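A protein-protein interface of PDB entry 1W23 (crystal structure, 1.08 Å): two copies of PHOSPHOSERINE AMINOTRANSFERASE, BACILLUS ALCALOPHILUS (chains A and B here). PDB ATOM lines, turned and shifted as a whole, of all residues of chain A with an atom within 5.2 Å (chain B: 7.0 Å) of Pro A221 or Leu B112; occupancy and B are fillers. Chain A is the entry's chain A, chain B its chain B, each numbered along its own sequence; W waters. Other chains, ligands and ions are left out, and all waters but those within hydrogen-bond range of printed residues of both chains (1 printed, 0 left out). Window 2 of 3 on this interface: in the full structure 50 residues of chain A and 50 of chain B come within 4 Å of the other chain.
Of the 15 printed residues of chain B, 7 touch a printed residue of chain A.
Hydrophobic or aromatic side chains of chain B that line the printed part of chain A: Leu B78, Met B85, Leu B112 and Leu B224.
Of the 7 printed residues of chain A, 4 touch a printed residue of chain B.
Hydrophobic or aromatic side chains of chain A within 4 Å of the printed part of chain B: Pro A221, Met A223 and Leu A224.
Among the printed residues, 8 pairs touch across the chains.
The side-chain amino group (NZ) of Lys B108 is in hydrogen-bond range of the side-chain hydroxyl (OG1) of Thr A222 (3.0 Å).
OG1 of Thr A222 is in hydrogen-bond range of OE2 of Glu B109, at 2.6 Å.
Among the printed residues, merely in contact across the chains: Pro A221 with Thr B81, Pro A221 with Glu B109, Leu A224 with Leu B224, Pro A221 with Leu B112, Pro A221 with Met B85 and Met A223 with Leu B78.
Water W1 lies within hydrogen-bond range of the backbone NH of Met A223 (2.8 Å), the side-chain carboxylate of Glu B109 (2.9 Å) and the backbone NH of Thr A222 (3.2 Å).
Leu B224 touches its own counterpart, Leu A224.
The side-chain amino group (NZ) of Lys B108 lies within salt-bridge range of the side-chain carboxylate (OE2) of Glu B109 (3.5 Å).
Val A220 touches none of the printed residues of chain B.
Of the printed residues of chain B, Pro A221 touches Thr B81, Met B85, Glu B109 and Leu B112.
Of the printed residues of chain B, Thr A222 touches Lys B108 and Glu B109.
Of the printed residues of chain B, Leu A224 touches Leu B224.
Printed residues of chain A within 4 Å of Thr B81: Pro A221.
Printed residues of chain A within 4 Å of Met B85: Pro A221 (3.99 Å).
Of the printed residues of chain A, Glu B109 touches Pro A221 (3.8 Å) and Thr A222 (2.6 Å).
Of the printed residues of chain A, Leu B112 touches Pro A221 (3.99 Å).
The nearest printed residue of chain B that does not touch Pro A221 is Leu B113 (4.7 Å).
The nearest printed residue of chain A that does not touch Leu B112 is Val A220 (4.3 Å).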
ATOM      1  N   GLN A 219     -15.481  -4.088 -12.343  1.00  0.00           N
ATOM      2  CA  GLN A 219     -15.713  -5.486 -12.034  1.00  0.00           C
ATOM      3  C   GLN A 219     -17.163  -5.919 -12.194  1.00  0.00           C
ATOM      4  O   GLN A 219     -17.454  -7.107 -11.959  1.00  0.00           O
ATOM      5  CB  GLN A 219     -15.274  -5.821 -10.605  1.00  0.00           C
ATOM      6  N   VAL A 220     -18.063  -5.037 -12.586  1.00  0.00           N
ATOM      7  CA  VAL A 220     -19.432  -5.489 -12.848  1.00  0.00           C
ATOM      8  C   VAL A 220     -19.593  -5.880 -14.318  1.00  0.00           C
ATOM      9  O   VAL A 220     -19.150  -5.104 -15.182  1.00  0.00           O
ATOM     10  CB  VAL A 220     -20.419  -4.379 -12.443  1.00  0.00           C
ATOM     11  CG1 VAL A 220     -21.849  -4.736 -12.844  1.00  0.00           C
ATOM     12  CG2 VAL A 220     -20.322  -4.143 -10.919  1.00  0.00           C
ATOM     13  N   PRO A 221     -20.181  -7.034 -14.649  1.00  0.00           N
ATOM     14  CA  PRO A 221     -20.386  -7.415 -16.050  1.00  0.00           C
ATOM     15  C   PRO A 221     -21.070  -6.304 -16.836  1.00  0.00           C
ATOM     16  O   PRO A 221     -21.958  -5.597 -16.325  1.00  0.00           O
ATOM     17  CB  PRO A 221     -21.292  -8.593 -15.938  1.00  0.00           C
ATOM     18  CG  PRO A 221     -20.825  -9.239 -14.655  1.00  0.00           C
ATOM     19  CD  PRO A 221     -20.641  -8.062 -13.722  1.00  0.00           C
ATOM     20  N   THR A 222     -20.748  -6.222 -18.136  1.00  0.00           N
ATOM     21  CA  THR A 222     -21.250  -5.164 -19.001  1.00  0.00           C
ATOM     22  C   THR A 222     -22.765  -5.004 -18.930  1.00  0.00           C
ATOM     23  O   THR A 222     -23.303  -3.876 -18.782  1.00  0.00           O
ATOM     24  CB  THR A 222     -20.802  -5.481 -20.458  1.00  0.00           C
ATOM     25  OG1 THR A 222     -19.387  -5.675 -20.500  1.00  0.00           O
ATOM     26  CG2 THR A 222     -21.145  -4.284 -21.316  1.00  0.00           C
ATOM     27  N   MET A 223     -23.483  -6.105 -19.070  1.00  0.00           N
ATOM     28  CA  MET A 223     -24.964  -6.052 -19.129  1.00  0.00           C
ATOM     29  C   MET A 223     -25.540  -5.627 -17.790  1.00  0.00           C
ATOM     30  O   MET A 223     -26.717  -5.217 -17.773  1.00  0.00           O
ATOM     31  CB  MET A 223     -25.553  -7.417 -19.515  1.00  0.00           C
ATOM     32  CG  MET A 223     -25.610  -7.708 -21.015  1.00  0.00           C
ATOM     33  SD  MET A 223     -26.769  -6.625 -21.899  1.00  0.00           S
ATOM     34  CE  MET A 223     -28.350  -7.228 -21.328  1.00  0.00           C
ATOM     35  N   LEU A 224     -24.804  -5.728 -16.689  1.00  0.00           N
ATOM     36  CA  LEU A 224     -25.295  -5.453 -15.343  1.00  0.00           C
ATOM     37  C   LEU A 224     -24.919  -4.064 -14.848  1.00  0.00           C
ATOM     38  O   LEU A 224     -25.284  -3.740 -13.701  1.00  0.00           O
ATOM     39  CB  LEU A 224     -24.878  -6.542 -14.364  1.00  0.00           C
ATOM     40  CG  LEU A 224     -25.549  -7.912 -14.667  1.00  0.00           C
ATOM     41  CD1 LEU A 224     -24.814  -9.047 -14.005  1.00  0.00           C
ATOM     42  CD2 LEU A 224     -27.004  -7.847 -14.216  1.00  0.00           C
ATOM     43  N   GLN A 225     -24.245  -3.270 -15.644  1.00  0.00           N
ATOM     44  CA  GLN A 225     -23.949  -1.849 -15.345  1.00  0.00           C
ATOM     45  C   GLN A 225     -25.059  -0.954 -15.794  1.00  0.00           C
ATOM     46  O   GLN A 225     -25.396  -0.990 -16.974  1.00  0.00           O
ATOM     47  CB  GLN A 225     -22.628  -1.392 -16.017  1.00  0.00           C
ATOM     48  CG  GLN A 225     -21.440  -2.169 -15.568  1.00  0.00           C
ATOM     49  CD  GLN A 225     -20.161  -1.527 -15.869  1.00  0.00           C
ATOM     50  OE1 GLN A 225     -20.129  -0.379 -16.315  1.00  0.00           O
ATOM     51  NE2 GLN A 225     -19.142  -2.286 -15.596  1.00  0.00           N
ATOM     52  N   LEU B  78     -26.706 -11.445 -22.142  1.00  0.00           N
ATOM     53  CA  LEU B  78     -26.657 -11.768 -20.698  1.00  0.00           C
ATOM     54  C   LEU B  78     -26.071 -13.129 -20.495  1.00  0.00           C
ATOM     55  O   LEU B  78     -25.369 -13.365 -19.467  1.00  0.00           O
ATOM     56  CB  LEU B  78     -28.023 -11.632 -20.037  1.00  0.00           C
ATOM     57  CG  LEU B  78     -28.016 -11.767 -18.513  1.00  0.00           C
ATOM     58  CD1 LEU B  78     -27.258 -10.625 -17.852  1.00  0.00           C
ATOM     59  CD2 LEU B  78     -29.422 -11.796 -17.952  1.00  0.00           C
ATOM     60  N   THR B  81     -22.245 -13.432 -19.758  1.00  0.00           N
ATOM     61  CA  THR B  81     -21.794 -13.331 -18.359  1.00  0.00           C
ATOM     62  C   THR B  81     -22.390 -14.429 -17.503  1.00  0.00           C
ATOM     63  O   THR B  81     -21.681 -14.969 -16.592  1.00  0.00           O
ATOM     64  CB  THR B  81     -22.023 -11.912 -17.809  1.00  0.00           C
ATOM     65  OG1 THR B  81     -21.336 -11.866 -16.513  1.00  0.00           O
ATOM     66  CG2 THR B  81     -23.448 -11.593 -17.550  1.00  0.00           C
ATOM     67  N   MET B  82     -23.645 -14.804 -17.684  1.00  0.00           N
ATOM     68  CA  MET B  82     -24.258 -15.798 -16.808  1.00  0.00           C
ATOM     69  C   MET B  82     -23.532 -17.129 -16.898  1.00  0.00           C
ATOM     70  O   MET B  82     -23.383 -17.831 -15.878  1.00  0.00           O
ATOM     71  CB  MET B  82     -25.753 -15.909 -17.142  1.00  0.00           C
ATOM     72  CG  MET B  82     -26.556 -16.643 -16.124  1.00  0.00           C
ATOM     73  SD  MET B  82     -28.322 -16.452 -16.504  1.00  0.00           S
ATOM     74  CE  MET B  82     -28.989 -17.687 -15.414  1.00  0.00           C
ATOM     75  N   MET B  85     -20.335 -16.970 -14.867  1.00  0.00           N
ATOM     76  CA  MET B  85     -20.683 -16.762 -13.473  1.00  0.00           C
ATOM     77  C   MET B  85     -21.052 -18.082 -12.790  1.00  0.00           C
ATOM     78  O   MET B  85     -20.800 -18.265 -11.612  1.00  0.00           O
ATOM     79  CB  MET B  85     -21.778 -15.708 -13.444  1.00  0.00           C
ATOM     80  CG  MET B  85     -21.958 -15.035 -12.109  1.00  0.00           C
ATOM     81  SD  MET B  85     -23.242 -13.789 -12.081  1.00  0.00           S
ATOM     82  CE  MET B  85     -22.607 -12.472 -13.137  1.00  0.00           C
ATOM     83  N   LEU B  88     -17.415 -20.916 -14.427  1.00  0.00           N
ATOM     84  CA  LEU B  88     -15.991 -20.555 -14.435  1.00  0.00           C
ATOM     85  C   LEU B  88     -15.544 -20.383 -13.004  1.00  0.00           C
ATOM     86  O   LEU B  88     -15.544 -19.298 -12.447  1.00  0.00           O
ATOM     87  CB  LEU B  88     -15.731 -19.303 -15.302  1.00  0.00           C
ATOM     88  CG  LEU B  88     -14.278 -18.889 -15.495  1.00  0.00           C
ATOM     89  CD1 LEU B  88     -13.414 -20.085 -15.913  1.00  0.00           C
ATOM     90  CD2 LEU B  88     -14.147 -17.775 -16.523  1.00  0.00           C
ATOM     91  N   LEU B 107     -16.058 -13.992 -24.997  1.00  0.00           N
ATOM     92  CA  LEU B 107     -14.769 -14.132 -24.297  1.00  0.00           C
ATOM     93  C   LEU B 107     -14.534 -12.958 -23.352  1.00  0.00           C
ATOM     94  O   LEU B 107     -14.077 -13.121 -22.224  1.00  0.00           O
ATOM     95  CB  LEU B 107     -13.642 -14.202 -25.337  1.00  0.00           C
ATOM     96  CG  LEU B 107     -12.211 -14.050 -24.820  1.00  0.00           C
ATOM     97  CD1 LEU B 107     -11.891 -15.173 -23.846  1.00  0.00           C
ATOM     98  CD2 LEU B 107     -11.237 -14.047 -25.998  1.00  0.00           C
ATOM     99  N   LYS B 108     -14.863 -11.741 -23.810  1.00  0.00           N
ATOM    100  CA  LYS B 108     -14.670 -10.513 -23.044  1.00  0.00           C
ATOM    101  C   LYS B 108     -15.359 -10.621 -21.686  1.00  0.00           C
ATOM    102  O   LYS B 108     -14.818 -10.210 -20.636  1.00  0.00           O
ATOM    103  CB  LYS B 108     -15.163  -9.310 -23.810  1.00  0.00           C
ATOM    104  CG  LYS B 108     -15.151  -7.999 -23.043  1.00  0.00           C
ATOM    105  CD  LYS B 108     -15.621  -6.837 -23.873  1.00  0.00           C
ATOM    106  CE  LYS B 108     -15.737  -5.588 -23.029  1.00  0.00           C
ATOM    107  NZ  LYS B 108     -17.027  -5.280 -22.366  1.00  0.00           N
ATOM    108  N   GLU B 109     -16.598 -11.117 -21.647  1.00  0.00           N
ATOM    109  CA  GLU B 109     -17.316 -11.188 -20.383  1.00  0.00           C
ATOM    110  C   GLU B 109     -16.711 -12.243 -19.468  1.00  0.00           C
ATOM    111  O   GLU B 109     -16.693 -12.043 -18.252  1.00  0.00           O
ATOM    112  CB  GLU B 109     -18.804 -11.463 -20.619  1.00  0.00           C
ATOM    113  CG  GLU B 109     -19.516 -10.349 -21.360  1.00  0.00           C
ATOM    114  CD  GLU B 109     -19.332  -9.000 -20.672  1.00  0.00           C
ATOM    115  OE1 GLU B 109     -19.529  -8.874 -19.435  1.00  0.00           O
ATOM    116  OE2 GLU B 109     -18.968  -8.087 -21.417  1.00  0.00           O
ATOM    117  N   ALA B 110     -16.213 -13.358 -20.018  1.00  0.00           N
ATOM    118  CA  ALA B 110     -15.570 -14.378 -19.172  1.00  0.00           C
ATOM    119  C   ALA B 110     -14.301 -13.819 -18.535  1.00  0.00           C
ATOM    120  O   ALA B 110     -13.995 -14.170 -17.391  1.00  0.00           O
ATOM    121  CB  ALA B 110     -15.325 -15.651 -19.934  1.00  0.00           C
ATOM    122  N   LYS B 111     -13.582 -12.971 -19.244  1.00  0.00           N
ATOM    123  CA  LYS B 111     -12.314 -12.452 -18.740  1.00  0.00           C
ATOM    124  C   LYS B 111     -12.497 -11.624 -17.478  1.00  0.00           C
ATOM    125  O   LYS B 111     -11.600 -11.495 -16.647  1.00  0.00           O
ATOM    126  CB  LYS B 111     -11.637 -11.673 -19.848  1.00  0.00           C
ATOM    127  CG  LYS B 111     -10.135 -11.534 -19.752  1.00  0.00           C
ATOM    128  CD  LYS B 111      -9.604 -11.157 -21.146  1.00  0.00           C
ATOM    129  CE  LYS B 111      -8.762 -12.261 -21.780  1.00  0.00           C
ATOM    130  NZ  LYS B 111      -8.555 -11.974 -23.233  1.00  0.00           N
ATOM    131  N   LEU B 112     -13.663 -11.020 -17.285  1.00  0.00           N
ATOM    132  CA  LEU B 112     -13.943 -10.279 -16.090  1.00  0.00           C
ATOM    133  C   LEU B 112     -14.097 -11.193 -14.888  1.00  0.00           C
ATOM    134  O   LEU B 112     -13.902 -10.791 -13.751  1.00  0.00           O
ATOM    135  CB  LEU B 112     -15.264  -9.495 -16.254  1.00  0.00           C
ATOM    136  CG  LEU B 112     -15.336  -8.340 -17.251  1.00  0.00           C
ATOM    137  CD1 LEU B 112     -16.685  -7.691 -17.515  1.00  0.00           C
ATOM    138  CD2 LEU B 112     -14.370  -7.231 -16.764  1.00  0.00           C
ATOM    139  N   LEU B 113     -14.431 -12.454 -15.116  1.00  0.00           N
ATOM    140  CA  LEU B 113     -14.791 -13.355 -14.040  1.00  0.00           C
ATOM    141  C   LEU B 113     -13.801 -14.451 -13.744  1.00  0.00           C
ATOM    142  O   LEU B 113     -13.861 -15.125 -12.685  1.00  0.00           O
ATOM    143  CB  LEU B 113     -16.123 -13.950 -14.364  1.00  0.00           C
ATOM    144  CG  LEU B 113     -17.263 -12.945 -14.522  1.00  0.00           C
ATOM    145  CD1 LEU B 113     -18.502 -13.629 -15.040  1.00  0.00           C
ATOM    146  CD2 LEU B 113     -17.540 -12.220 -13.226  1.00  0.00           C
ATOM    147  N   GLY B 114     -12.848 -14.727 -14.604  1.00  0.00           N
ATOM    148  CA  GLY B 114     -11.868 -15.766 -14.299  1.00  0.00           C
ATOM    149  C   GLY B 114     -10.859 -15.928 -15.420  1.00  0.00           C
ATOM    150  O   GLY B 114     -10.788 -15.090 -16.322  1.00  0.00           O
ATOM    151  N   THR B 116      -9.209 -17.223 -18.765  1.00  0.00           N
ATOM    152  CA  THR B 116      -9.683 -17.565 -20.078  1.00  0.00           C
ATOM    153  C   THR B 116      -8.511 -17.985 -20.964  1.00  0.00           C
ATOM    154  O   THR B 116      -7.324 -17.842 -20.609  1.00  0.00           O
ATOM    155  CB  THR B 116     -10.429 -16.399 -20.742  1.00  0.00           C
ATOM    156  OG1 THR B 116      -9.535 -15.267 -20.898  1.00  0.00           O
ATOM    157  CG2 THR B 116     -11.652 -16.000 -19.937  1.00  0.00           C
ATOM    158  N   LEU B 224     -29.378 -14.929 -11.432  1.00  0.00           N
ATOM    159  CA  LEU B 224     -28.231 -15.247 -12.299  1.00  0.00           C
ATOM    160  C   LEU B 224     -27.741 -16.673 -12.102  1.00  0.00           C
ATOM    161  O   LEU B 224     -26.799 -17.059 -12.778  1.00  0.00           O
ATOM    162  CB  LEU B 224     -27.118 -14.220 -12.082  1.00  0.00           C
ATOM    163  CG  LEU B 224     -27.457 -12.843 -12.597  1.00  0.00           C
ATOM    164  CD1 LEU B 224     -26.564 -11.785 -12.048  1.00  0.00           C
ATOM    165  CD2 LEU B 224     -27.347 -12.854 -14.137  1.00  0.00           C
HETATM  166  O   HOH W   1     -22.403  -8.682 -19.456  1.00  0.00           O
